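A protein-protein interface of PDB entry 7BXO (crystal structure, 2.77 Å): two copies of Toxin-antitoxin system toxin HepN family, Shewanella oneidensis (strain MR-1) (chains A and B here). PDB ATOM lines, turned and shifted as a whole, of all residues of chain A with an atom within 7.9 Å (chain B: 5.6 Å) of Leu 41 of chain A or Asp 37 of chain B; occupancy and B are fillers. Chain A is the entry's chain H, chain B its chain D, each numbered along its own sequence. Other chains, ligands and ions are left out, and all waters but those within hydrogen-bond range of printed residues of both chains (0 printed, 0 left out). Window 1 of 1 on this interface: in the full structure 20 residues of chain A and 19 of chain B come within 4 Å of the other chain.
Hydrophobic or aromatic side chains of chain B within 4 Å of the printed part of chain A: Phe 33, Leu 41, Ala 100 and Val 101.
Leu 35 of chain A touches Thr 34 of chain B, but with the chains exchanged Thr 34 of chain A does not touch Leu 35 of chain B (4.7 Å). Asp 37 of chain A touches Asn 42 of chain B, and with the chains exchanged Asn 42 of chain A touches Asp 37 of chain B. Leu 41 of chain A touches Ala 100 of chain B, and with the chains exchanged Ala 100 of chain A touches Leu 41 of chain B. Gln 44 of chain B touches its own counterpart, Gln 44 of chain A.
O of Asn 42 of chain A is in hydrogen-bond range of SG of Cys 46 of chain A (3.4 Å). The side-chain amide oxygen of Asn 42 of chain A lies within hydrogen-bond range of the guanidinium group of Arg 45 of chain A, 3.2 Å away. ND2 of Asn 42 of chain A sits at hydrogen-bond distance from O of Ser 38 of chain A, at 3.0 Å. The backbone carbonyl oxygen of Ser 38 of chain B is in hydrogen-bond range of the side-chain amide nitrogen of Asn 42 of chain B, 2.9 Å away. SG of Cys 15 of chain A is in hydrogen-bond range of OD1 of Asn 42 of chain A, 3.6 Å away.
OD2 of Asp 37 of chain B is in hydrogen-bond range of OG of Ser 38 of chain A (2.7 Å). OD2 of Asp 37 of chain B is in hydrogen-bond range of ND2 of Asn 42 of chain A (3.4 Å). The side-chain hydroxyl of Ser 38 of chain B sits at hydrogen-bond distance from the side-chain carboxylate of Asp 37 of chain A (3.0 Å). O of Ala 100 of chain B lies within hydrogen-bond range of NE of Arg 45 of chain A (3.0 Å). OD1 of Asp 37 of chain B lies within salt-bridge range of NH1 of Arg 45 of chain A, 3.1 Å away.
Phe 33 of chain B touches Val 22 of chain A. Thr 34 of chain B touches Val 22 of chain A (OG1 to CG2, 3.6 Å). Phe 33 of chain A touches Ser 38 of chain B. CG2 of Thr 34 of chain B touches CD2 of Leu 35 of chain A (3.9 Å). Leu 41 of chain B touches Asp 37 of chain A. CE1 of Phe 33 of chain B touches OG of Ser 38 of chain A (3.6 Å). O of Gln 44 of chain A touches CG1 of Val 101 of chain B, at 3.6 Å. Val 101 of chain B touches Arg 45 of chain A (CG1 to CA, 3.6 Å). Glu 48 of chain A touches Val 101 of chain B. Gln 44 of chain B touches Val 101 of chain A (NE2 to CG1, 3.5 Å).
Of the printed residues of chain B, Leu 41 of chain A touches Asp 37 (3.5 Å) and Ala 100 (3.8 Å). Asp 37 of chain B touches just these residues of chain A: Ser 38, Leu 41, Asn 42 and Arg 45. Of the printed residues of chain B, Ser 38 of chain A touches Phe 33 (3.6 Å) and Asp 37 (2.7 Å). Of the printed residues of chain B, Ile 40 of chain A touches Leu 41. Of the printed residues of chain A, Asn 42 of chain B touches Asp 37. Of the printed residues of chain B, Leu 35 of chain A touches Thr 34. Cys 15 of chain A touches none of the printed residues of chain B. The nearest printed residue of chain B that does not touch Leu 41 of chain A is Gln 44 of chain B (4.01 Å). The nearest printed residue of chain B that does not touch Asn 42 of chain A is Phe 33 of chain B (4.4 Å).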
ATOM      1  N   ARG A  14      23.069 -16.366 -21.419  1.00  0.00           N
ATOM      2  CA  ARG A  14      22.917 -16.829 -20.036  1.00  0.00           C
ATOM      3  C   ARG A  14      21.986 -18.038 -19.970  1.00  0.00           C
ATOM      4  O   ARG A  14      22.381 -19.061 -19.423  1.00  0.00           O
ATOM      5  CB  ARG A  14      22.403 -15.680 -19.148  1.00  0.00           C
ATOM      6  CG  ARG A  14      22.393 -15.954 -17.654  1.00  0.00           C
ATOM      7  CD  ARG A  14      22.360 -14.637 -16.911  1.00  0.00           C
ATOM      8  NE  ARG A  14      21.539 -14.686 -15.700  1.00  0.00           N
ATOM      9  CZ  ARG A  14      20.274 -14.282 -15.632  1.00  0.00           C
ATOM     10  NH1 ARG A  14      19.658 -13.816 -16.713  1.00  0.00           N
ATOM     11  NH2 ARG A  14      19.610 -14.354 -14.488  1.00  0.00           N
ATOM     12  N   CYS A  15      20.778 -17.929 -20.562  1.00  0.00           N
ATOM     13  CA  CYS A  15      19.763 -18.987 -20.597  1.00  0.00           C
ATOM     14  C   CYS A  15      20.251 -20.274 -21.276  1.00  0.00           C
ATOM     15  O   CYS A  15      19.972 -21.353 -20.756  1.00  0.00           O
ATOM     16  CB  CYS A  15      18.461 -18.483 -21.212  1.00  0.00           C
ATOM     17  SG  CYS A  15      17.682 -17.124 -20.300  1.00  0.00           S
ATOM     18  N   ARG A  18      22.662 -21.899 -18.974  1.00  0.00           N
ATOM     19  CA  ARG A  18      21.882 -22.458 -17.870  1.00  0.00           C
ATOM     20  C   ARG A  18      21.102 -23.714 -18.275  1.00  0.00           C
ATOM     21  O   ARG A  18      20.922 -24.588 -17.439  1.00  0.00           O
ATOM     22  CB  ARG A  18      20.980 -21.398 -17.229  1.00  0.00           C
ATOM     23  CG  ARG A  18      21.773 -20.376 -16.426  1.00  0.00           C
ATOM     24  CD  ARG A  18      20.903 -19.302 -15.834  1.00  0.00           C
ATOM     25  NE  ARG A  18      21.618 -18.539 -14.813  1.00  0.00           N
ATOM     26  CZ  ARG A  18      21.035 -17.981 -13.756  1.00  0.00           C
ATOM     27  NH1 ARG A  18      19.723 -18.079 -13.585  1.00  0.00           N
ATOM     28  NH2 ARG A  18      21.757 -17.313 -12.871  1.00  0.00           N
ATOM     29  N   ILE A  19      20.653 -23.820 -19.544  1.00  0.00           N
ATOM     30  CA  ILE A  19      19.944 -25.007 -20.050  1.00  0.00           C
ATOM     31  C   ILE A  19      20.953 -26.166 -20.156  1.00  0.00           C
ATOM     32  O   ILE A  19      20.716 -27.236 -19.595  1.00  0.00           O
ATOM     33  CB  ILE A  19      19.187 -24.725 -21.395  1.00  0.00           C
ATOM     34  CG1 ILE A  19      17.936 -23.858 -21.162  1.00  0.00           C
ATOM     35  CG2 ILE A  19      18.806 -26.028 -22.127  1.00  0.00           C
ATOM     36  CD1 ILE A  19      17.519 -22.990 -22.357  1.00  0.00           C
ATOM     37  N   VAL A  22      22.097 -27.294 -16.531  1.00  0.00           N
ATOM     38  CA  VAL A  22      21.006 -28.024 -15.881  1.00  0.00           C
ATOM     39  C   VAL A  22      20.752 -29.410 -16.536  1.00  0.00           C
ATOM     40  O   VAL A  22      20.670 -30.406 -15.813  1.00  0.00           O
ATOM     41  CB  VAL A  22      19.731 -27.142 -15.793  1.00  0.00           C
ATOM     42  CG1 VAL A  22      18.477 -27.970 -15.572  1.00  0.00           C
ATOM     43  CG2 VAL A  22      19.870 -26.089 -14.699  1.00  0.00           C
ATOM     44  N   PHE A  33      11.858 -32.744 -11.501  1.00  0.00           N
ATOM     45  CA  PHE A  33      10.959 -31.768 -12.127  1.00  0.00           C
ATOM     46  C   PHE A  33      11.492 -30.335 -12.071  1.00  0.00           C
ATOM     47  O   PHE A  33      11.119 -29.539 -12.926  1.00  0.00           O
ATOM     48  CB  PHE A  33       9.510 -31.853 -11.593  1.00  0.00           C
ATOM     49  CG  PHE A  33       9.240 -31.443 -10.162  1.00  0.00           C
ATOM     50  CD1 PHE A  33       9.342 -30.112  -9.769  1.00  0.00           C
ATOM     51  CD2 PHE A  33       8.772 -32.366  -9.236  1.00  0.00           C
ATOM     52  CE1 PHE A  33       9.070 -29.730  -8.456  1.00  0.00           C
ATOM     53  CE2 PHE A  33       8.481 -31.977  -7.923  1.00  0.00           C
ATOM     54  CZ  PHE A  33       8.637 -30.663  -7.542  1.00  0.00           C
ATOM     55  N   THR A  34      12.360 -30.012 -11.088  1.00  0.00           N
ATOM     56  CA  THR A  34      12.953 -28.672 -10.925  1.00  0.00           C
ATOM     57  C   THR A  34      13.931 -28.356 -12.062  1.00  0.00           C
ATOM     58  O   THR A  34      14.092 -27.191 -12.427  1.00  0.00           O
ATOM     59  CB  THR A  34      13.602 -28.503  -9.545  1.00  0.00           C
ATOM     60  OG1 THR A  34      14.728 -29.371  -9.435  1.00  0.00           O
ATOM     61  CG2 THR A  34      12.644 -28.768  -8.409  1.00  0.00           C
ATOM     62  N   LEU A  35      14.583 -29.402 -12.610  1.00  0.00           N
ATOM     63  CA  LEU A  35      15.511 -29.297 -13.733  1.00  0.00           C
ATOM     64  C   LEU A  35      14.715 -29.084 -15.015  1.00  0.00           C
ATOM     65  O   LEU A  35      15.121 -28.281 -15.858  1.00  0.00           O
ATOM     66  CB  LEU A  35      16.371 -30.568 -13.864  1.00  0.00           C
ATOM     67  CG  LEU A  35      17.267 -30.968 -12.689  1.00  0.00           C
ATOM     68  CD1 LEU A  35      17.979 -32.255 -12.996  1.00  0.00           C
ATOM     69  CD2 LEU A  35      18.283 -29.881 -12.341  1.00  0.00           C
ATOM     70  N   GLN A  36      13.578 -29.812 -15.152  1.00  0.00           N
ATOM     71  CA  GLN A  36      12.642 -29.730 -16.281  1.00  0.00           C
ATOM     72  C   GLN A  36      12.082 -28.321 -16.341  1.00  0.00           C
ATOM     73  O   GLN A  36      12.162 -27.681 -17.387  1.00  0.00           O
ATOM     74  CB  GLN A  36      11.494 -30.736 -16.104  1.00  0.00           C
ATOM     75  CG  GLN A  36      11.917 -32.187 -16.276  1.00  0.00           C
ATOM     76  CD  GLN A  36      11.006 -33.156 -15.567  1.00  0.00           C
ATOM     77  OE1 GLN A  36       9.784 -32.972 -15.485  1.00  0.00           O
ATOM     78  NE2 GLN A  36      11.589 -34.225 -15.050  1.00  0.00           N
ATOM     79  N   ASP A  37      11.589 -27.821 -15.186  1.00  0.00           N
ATOM     80  CA  ASP A  37      11.026 -26.488 -15.003  1.00  0.00           C
ATOM     81  C   ASP A  37      12.003 -25.370 -15.341  1.00  0.00           C
ATOM     82  O   ASP A  37      11.601 -24.409 -15.990  1.00  0.00           O
ATOM     83  CB  ASP A  37      10.449 -26.322 -13.588  1.00  0.00           C
ATOM     84  CG  ASP A  37       9.190 -27.129 -13.311  1.00  0.00           C
ATOM     85  OD1 ASP A  37       8.585 -27.644 -14.282  1.00  0.00           O
ATOM     86  OD2 ASP A  37       8.813 -27.256 -12.119  1.00  0.00           O
ATOM     87  N   SER A  38      13.284 -25.511 -14.941  1.00  0.00           N
ATOM     88  CA  SER A  38      14.346 -24.544 -15.227  1.00  0.00           C
ATOM     89  C   SER A  38      14.613 -24.474 -16.726  1.00  0.00           C
ATOM     90  O   SER A  38      14.617 -23.378 -17.291  1.00  0.00           O
ATOM     91  CB  SER A  38      15.621 -24.896 -14.468  1.00  0.00           C
ATOM     92  OG  SER A  38      16.634 -23.929 -14.699  1.00  0.00           O
ATOM     93  N   VAL A  39      14.806 -25.647 -17.371  1.00  0.00           N
ATOM     94  CA  VAL A  39      15.035 -25.768 -18.814  1.00  0.00           C
ATOM     95  C   VAL A  39      13.866 -25.145 -19.600  1.00  0.00           C
ATOM     96  O   VAL A  39      14.107 -24.347 -20.506  1.00  0.00           O
ATOM     97  CB  VAL A  39      15.337 -27.235 -19.223  1.00  0.00           C
ATOM     98  CG1 VAL A  39      15.096 -27.466 -20.706  1.00  0.00           C
ATOM     99  CG2 VAL A  39      16.765 -27.617 -18.856  1.00  0.00           C
ATOM    100  N   ILE A  40      12.613 -25.462 -19.201  1.00  0.00           N
ATOM    101  CA  ILE A  40      11.387 -24.954 -19.822  1.00  0.00           C
ATOM    102  C   ILE A  40      11.298 -23.418 -19.724  1.00  0.00           C
ATOM    103  O   ILE A  40      11.148 -22.757 -20.756  1.00  0.00           O
ATOM    104  CB  ILE A  40      10.136 -25.685 -19.267  1.00  0.00           C
ATOM    105  CG1 ILE A  40      10.056 -27.128 -19.810  1.00  0.00           C
ATOM    106  CG2 ILE A  40       8.869 -24.927 -19.606  1.00  0.00           C
ATOM    107  CD1 ILE A  40       9.269 -28.123 -18.925  1.00  0.00           C
ATOM    108  N   LEU A  41      11.431 -22.864 -18.496  1.00  0.00           N
ATOM    109  CA  LEU A  41      11.394 -21.424 -18.232  1.00  0.00           C
ATOM    110  C   LEU A  41      12.485 -20.671 -18.997  1.00  0.00           C
ATOM    111  O   LEU A  41      12.198 -19.625 -19.577  1.00  0.00           O
ATOM    112  CB  LEU A  41      11.479 -21.145 -16.724  1.00  0.00           C
ATOM    113  CG  LEU A  41      11.162 -19.717 -16.251  1.00  0.00           C
ATOM    114  CD1 LEU A  41       9.699 -19.341 -16.504  1.00  0.00           C
ATOM    115  CD2 LEU A  41      11.455 -19.579 -14.786  1.00  0.00           C
ATOM    116  N   ASN A  42      13.714 -21.223 -19.040  1.00  0.00           N
ATOM    117  CA  ASN A  42      14.829 -20.621 -19.774  1.00  0.00           C
ATOM    118  C   ASN A  42      14.642 -20.696 -21.287  1.00  0.00           C
ATOM    119  O   ASN A  42      15.169 -19.842 -22.000  1.00  0.00           O
ATOM    120  CB  ASN A  42      16.176 -21.189 -19.335  1.00  0.00           C
ATOM    121  CG  ASN A  42      16.652 -20.672 -18.001  1.00  0.00           C
ATOM    122  OD1 ASN A  42      16.741 -19.461 -17.769  1.00  0.00           O
ATOM    123  ND2 ASN A  42      16.985 -21.583 -17.098  1.00  0.00           N
ATOM    124  N   LEU A  43      13.862 -21.679 -21.784  1.00  0.00           N
ATOM    125  CA  LEU A  43      13.570 -21.756 -23.219  1.00  0.00           C
ATOM    126  C   LEU A  43      12.626 -20.608 -23.596  1.00  0.00           C
ATOM    127  O   LEU A  43      12.915 -19.883 -24.550  1.00  0.00           O
ATOM    128  CB  LEU A  43      12.995 -23.121 -23.638  1.00  0.00           C
ATOM    129  CG  LEU A  43      13.996 -24.280 -23.777  1.00  0.00           C
ATOM    130  CD1 LEU A  43      13.270 -25.625 -23.792  1.00  0.00           C
ATOM    131  CD2 LEU A  43      14.885 -24.113 -25.002  1.00  0.00           C
ATOM    132  N   GLN A  44      11.562 -20.383 -22.781  1.00  0.00           N
ATOM    133  CA  GLN A  44      10.601 -19.282 -22.936  1.00  0.00           C
ATOM    134  C   GLN A  44      11.319 -17.932 -22.873  1.00  0.00           C
ATOM    135  O   GLN A  44      10.952 -17.013 -23.602  1.00  0.00           O
ATOM    136  CB  GLN A  44       9.544 -19.328 -21.831  1.00  0.00           C
ATOM    137  CG  GLN A  44       8.495 -20.424 -21.993  1.00  0.00           C
ATOM    138  CD  GLN A  44       7.582 -20.557 -20.789  1.00  0.00           C
ATOM    139  OE1 GLN A  44       7.434 -19.648 -19.954  1.00  0.00           O
ATOM    140  NE2 GLN A  44       6.935 -21.702 -20.684  1.00  0.00           N
ATOM    141  N   ARG A  45      12.341 -17.820 -22.000  1.00  0.00           N
ATOM    142  CA  ARG A  45      13.158 -16.622 -21.835  1.00  0.00           C
ATOM    143  C   ARG A  45      13.962 -16.318 -23.098  1.00  0.00           C
ATOM    144  O   ARG A  45      14.084 -15.148 -23.452  1.00  0.00           O
ATOM    145  CB  ARG A  45      14.076 -16.748 -20.616  1.00  0.00           C
ATOM    146  CG  ARG A  45      13.384 -16.557 -19.273  1.00  0.00           C
ATOM    147  CD  ARG A  45      14.401 -16.601 -18.144  1.00  0.00           C
ATOM    148  NE  ARG A  45      13.805 -16.300 -16.839  1.00  0.00           N
ATOM    149  CZ  ARG A  45      13.891 -17.089 -15.772  1.00  0.00           C
ATOM    150  NH1 ARG A  45      14.545 -18.240 -15.840  1.00  0.00           N
ATOM    151  NH2 ARG A  45      13.319 -16.733 -14.629  1.00  0.00           N
ATOM    152  N   CYS A  46      14.495 -17.366 -23.784  1.00  0.00           N
ATOM    153  CA  CYS A  46      15.261 -17.250 -25.039  1.00  0.00           C
ATOM    154  C   CYS A  46      14.306 -16.793 -26.132  1.00  0.00           C
ATOM    155  O   CYS A  46      14.646 -15.931 -26.948  1.00  0.00           O
ATOM    156  CB  CYS A  46      15.902 -18.582 -25.422  1.00  0.00           C
ATOM    157  SG  CYS A  46      17.340 -19.062 -24.433  1.00  0.00           S
ATOM    158  N   CYS A  47      13.104 -17.399 -26.144  1.00  0.00           N
ATOM    159  CA  CYS A  47      12.054 -17.115 -27.106  1.00  0.00           C
ATOM    160  C   CYS A  47      11.592 -15.670 -27.050  1.00  0.00           C
ATOM    161  O   CYS A  47      11.584 -15.010 -28.086  1.00  0.00           O
ATOM    162  CB  CYS A  47      10.894 -18.087 -26.945  1.00  0.00           C
ATOM    163  SG  CYS A  47       9.638 -17.938 -28.235  1.00  0.00           S
ATOM    164  N   GLU A  48      11.256 -15.157 -25.844  1.00  0.00           N
ATOM    165  CA  GLU A  48      10.824 -13.769 -25.668  1.00  0.00           C
ATOM    166  C   GLU A  48      11.941 -12.772 -25.909  1.00  0.00           C
ATOM    167  O   GLU A  48      11.667 -11.690 -26.420  1.00  0.00           O
ATOM    168  CB  GLU A  48      10.139 -13.525 -24.320  1.00  0.00           C
ATOM    169  CG  GLU A  48       8.777 -14.196 -24.172  1.00  0.00           C
ATOM    170  CD  GLU A  48       7.697 -13.877 -25.188  1.00  0.00           C
ATOM    171  OE1 GLU A  48       7.618 -12.716 -25.654  1.00  0.00           O
ATOM    172  OE2 GLU A  48       6.914 -14.801 -25.508  1.00  0.00           O
ATOM    173  N   ALA A 100       4.111 -25.314 -21.358  1.00  0.00           N
ATOM    174  CA  ALA A 100       4.332 -25.399 -19.919  1.00  0.00           C
ATOM    175  C   ALA A 100       3.132 -24.972 -19.092  1.00  0.00           C
ATOM    176  O   ALA A 100       2.521 -25.810 -18.425  1.00  0.00           O
ATOM    177  CB  ALA A 100       5.539 -24.574 -19.535  1.00  0.00           C
ATOM    178  N   VAL A 101       2.809 -23.662 -19.140  1.00  0.00           N
ATOM    179  CA  VAL A 101       1.758 -22.973 -18.383  1.00  0.00           C
ATOM    180  C   VAL A 101       0.386 -23.675 -18.465  1.00  0.00           C
ATOM    181  O   VAL A 101      -0.266 -23.845 -17.429  1.00  0.00           O
ATOM    182  CB  VAL A 101       1.662 -21.456 -18.729  1.00  0.00           C
ATOM    183  CG1 VAL A 101       2.943 -20.718 -18.350  1.00  0.00           C
ATOM    184  CG2 VAL A 101       1.308 -21.205 -20.194  1.00  0.00           C
ATOM    185  N   VAL A 112      10.895 -31.350 -25.173  1.00  0.00           N
ATOM    186  CA  VAL A 112      11.837 -30.493 -24.449  1.00  0.00           C
ATOM    187  C   VAL A 112      13.273 -30.922 -24.744  1.00  0.00           C
ATOM    188  O   VAL A 112      14.081 -30.078 -25.132  1.00  0.00           O
ATOM    189  CB  VAL A 112      11.543 -30.420 -22.928  1.00  0.00           C
ATOM    190  CG1 VAL A 112      12.298 -29.264 -22.283  1.00  0.00           C
ATOM    191  CG2 VAL A 112      10.049 -30.280 -22.662  1.00  0.00           C
ATOM    192  N   PHE B  33      19.260 -21.331  -8.669  1.00  0.00           N
ATOM    193  CA  PHE B  33      18.302 -20.766  -9.628  1.00  0.00           C
ATOM    194  C   PHE B  33      17.263 -21.801 -10.084  1.00  0.00           C
ATOM    195  O   PHE B  33      16.159 -21.426 -10.468  1.00  0.00           O
ATOM    196  CB  PHE B  33      19.005 -20.092 -10.824  1.00  0.00           C
ATOM    197  CG  PHE B  33      19.731 -20.996 -11.797  1.00  0.00           C
ATOM    198  CD1 PHE B  33      19.050 -21.612 -12.843  1.00  0.00           C
ATOM    199  CD2 PHE B  33      21.106 -21.170 -11.715  1.00  0.00           C
ATOM    200  CE1 PHE B  33      19.723 -22.434 -13.753  1.00  0.00           C
ATOM    201  CE2 PHE B  33      21.780 -21.984 -12.633  1.00  0.00           C
ATOM    202  CZ  PHE B  33      21.082 -22.614 -13.642  1.00  0.00           C
ATOM    203  N   THR B  34      17.629 -23.094 -10.037  1.00  0.00           N
ATOM    204  CA  THR B  34      16.805 -24.252 -10.393  1.00  0.00           C
ATOM    205  C   THR B  34      15.553 -24.292  -9.507  1.00  0.00           C
ATOM    206  O   THR B  34      14.460 -24.570 -10.000  1.00  0.00           O
ATOM    207  CB  THR B  34      17.687 -25.523 -10.319  1.00  0.00           C
ATOM    208  OG1 THR B  34      18.670 -25.456 -11.352  1.00  0.00           O
ATOM    209  CG2 THR B  34      16.901 -26.819 -10.445  1.00  0.00           C
ATOM    210  N   LEU B  35      15.719 -23.983  -8.212  1.00  0.00           N
ATOM    211  CA  LEU B  35      14.630 -23.949  -7.241  1.00  0.00           C
ATOM    212  C   LEU B  35      13.737 -22.725  -7.472  1.00  0.00           C
ATOM    213  O   LEU B  35      12.521 -22.823  -7.303  1.00  0.00           O
ATOM    214  CB  LEU B  35      15.175 -23.957  -5.801  1.00  0.00           C
ATOM    215  CG  LEU B  35      16.130 -25.092  -5.404  1.00  0.00           C
ATOM    216  CD1 LEU B  35      16.651 -24.879  -4.008  1.00  0.00           C
ATOM    217  CD2 LEU B  35      15.462 -26.457  -5.491  1.00  0.00           C
ATOM    218  N   GLN B  36      14.343 -21.579  -7.874  1.00  0.00           N
ATOM    219  CA  GLN B  36      13.643 -20.326  -8.186  1.00  0.00           C
ATOM    220  C   GLN B  36      12.786 -20.506  -9.442  1.00  0.00           C
ATOM    221  O   GLN B  36      11.619 -20.115  -9.443  1.00  0.00           O
ATOM    222  CB  GLN B  36      14.641 -19.177  -8.410  1.00  0.00           C
ATOM    223  CG  GLN B  36      15.378 -18.719  -7.162  1.00  0.00           C
ATOM    224  CD  GLN B  36      16.733 -18.138  -7.482  1.00  0.00           C
ATOM    225  OE1 GLN B  36      16.880 -17.230  -8.310  1.00  0.00           O
ATOM    226  NE2 GLN B  36      17.760 -18.653  -6.829  1.00  0.00           N
ATOM    227  N   ASP B  37      13.377 -21.108 -10.504  1.00  0.00           N
ATOM    228  CA  ASP B  37      12.752 -21.377 -11.800  1.00  0.00           C
ATOM    229  C   ASP B  37      11.517 -22.256 -11.699  1.00  0.00           C
ATOM    230  O   ASP B  37      10.524 -21.974 -12.366  1.00  0.00           O
ATOM    231  CB  ASP B  37      13.768 -21.980 -12.778  1.00  0.00           C
ATOM    232  CG  ASP B  37      14.782 -21.000 -13.341  1.00  0.00           C
ATOM    233  OD1 ASP B  37      14.603 -19.776 -13.145  1.00  0.00           O
ATOM    234  OD2 ASP B  37      15.752 -21.455 -13.985  1.00  0.00           O
ATOM    235  N   SER B  38      11.576 -23.297 -10.843  1.00  0.00           N
ATOM    236  CA  SER B  38      10.496 -24.243 -10.575  1.00  0.00           C
ATOM    237  C   SER B  38       9.299 -23.549  -9.917  1.00  0.00           C
ATOM    238  O   SER B  38       8.162 -23.764 -10.343  1.00  0.00           O
ATOM    239  CB  SER B  38      11.002 -25.388  -9.699  1.00  0.00           C
ATOM    240  OG  SER B  38      10.008 -26.375  -9.469  1.00  0.00           O
ATOM    241  N   VAL B  39       9.561 -22.711  -8.893  1.00  0.00           N
ATOM    242  CA  VAL B  39       8.546 -21.963  -8.145  1.00  0.00           C
ATOM    243  C   VAL B  39       7.792 -21.013  -9.082  1.00  0.00           C
ATOM    244  O   VAL B  39       6.560 -21.012  -9.078  1.00  0.00           O
ATOM    245  CB  VAL B  39       9.160 -21.247  -6.904  1.00  0.00           C
ATOM    246  CG1 VAL B  39       8.225 -20.183  -6.343  1.00  0.00           C
ATOM    247  CG2 VAL B  39       9.532 -22.251  -5.814  1.00  0.00           C
ATOM    248  N   ILE B  40       8.535 -20.240  -9.904  1.00  0.00           N
ATOM    249  CA  ILE B  40       7.976 -19.283 -10.862  1.00  0.00           C
ATOM    250  C   ILE B  40       7.083 -19.986 -11.889  1.00  0.00           C
ATOM    251  O   ILE B  40       5.952 -19.550 -12.104  1.00  0.00           O
ATOM    252  CB  ILE B  40       9.062 -18.409 -11.544  1.00  0.00           C
ATOM    253  CG1 ILE B  40       9.908 -17.614 -10.514  1.00  0.00           C
ATOM    254  CG2 ILE B  40       8.409 -17.465 -12.532  1.00  0.00           C
ATOM    255  CD1 ILE B  40      11.283 -17.023 -11.079  1.00  0.00           C
ATOM    256  N   LEU B  41       7.577 -21.069 -12.509  1.00  0.00           N
ATOM    257  CA  LEU B  41       6.807 -21.799 -13.502  1.00  0.00           C
ATOM    258  C   LEU B  41       5.509 -22.330 -12.901  1.00  0.00           C
ATOM    259  O   LEU B  41       4.447 -22.080 -13.463  1.00  0.00           O
ATOM    260  CB  LEU B  41       7.647 -22.903 -14.183  1.00  0.00           C
ATOM    261  CG  LEU B  41       7.077 -23.516 -15.476  1.00  0.00           C
ATOM    262  CD1 LEU B  41       6.979 -22.495 -16.605  1.00  0.00           C
ATOM    263  CD2 LEU B  41       7.904 -24.682 -15.926  1.00  0.00           C
ATOM    264  N   ASN B  42       5.580 -22.963 -11.718  1.00  0.00           N
ATOM    265  CA  ASN B  42       4.402 -23.484 -11.024  1.00  0.00           C
ATOM    266  C   ASN B  42       3.449 -22.374 -10.576  1.00  0.00           C
ATOM    267  O   ASN B  42       2.258 -22.639 -10.416  1.00  0.00           O
ATOM    268  CB  ASN B  42       4.788 -24.403  -9.870  1.00  0.00           C
ATOM    269  CG  ASN B  42       5.360 -25.723 -10.301  1.00  0.00           C
ATOM    270  OD1 ASN B  42       4.803 -26.429 -11.144  1.00  0.00           O
ATOM    271  ND2 ASN B  42       6.485 -26.095  -9.716  1.00  0.00           N
ATOM    272  N   GLN B  44       3.084 -19.490 -12.498  1.00  0.00           N
ATOM    273  CA  GLN B  44       2.533 -19.152 -13.819  1.00  0.00           C
ATOM    274  C   GLN B  44       1.435 -20.152 -14.211  1.00  0.00           C
ATOM    275  O   GLN B  44       0.449 -19.777 -14.848  1.00  0.00           O
ATOM    276  CB  GLN B  44       3.635 -19.173 -14.892  1.00  0.00           C
ATOM    277  CG  GLN B  44       4.671 -18.057 -14.770  1.00  0.00           C
ATOM    278  CD  GLN B  44       5.596 -17.917 -15.963  1.00  0.00           C
ATOM    279  OE1 GLN B  44       6.456 -17.037 -15.983  1.00  0.00           O
ATOM    280  NE2 GLN B  44       5.450 -18.757 -16.992  1.00  0.00           N
ATOM    281  N   ALA B 100       8.891 -13.474 -14.658  1.00  0.00           N
ATOM    282  CA  ALA B 100       9.952 -14.433 -14.965  1.00  0.00           C
ATOM    283  C   ALA B 100      10.711 -14.100 -16.227  1.00  0.00           C
ATOM    284  O   ALA B 100      11.936 -13.982 -16.206  1.00  0.00           O
ATOM    285  CB  ALA B 100       9.367 -15.821 -15.092  1.00  0.00           C
ATOM    286  N   VAL B 101       9.971 -13.962 -17.325  1.00  0.00           N
ATOM    287  CA  VAL B 101      10.498 -13.727 -18.654  1.00  0.00           C
ATOM    288  C   VAL B 101      11.036 -12.295 -18.826  1.00  0.00           C
ATOM    289  O   VAL B 101      12.236 -12.088 -18.646  1.00  0.00           O
ATOM    290  CB  VAL B 101       9.486 -14.130 -19.755  1.00  0.00           C
ATOM    291  CG1 VAL B 101      10.224 -14.643 -20.971  1.00  0.00           C
ATOM    292  CG2 VAL B 101       8.501 -15.189 -19.255  1.00  0.00           C
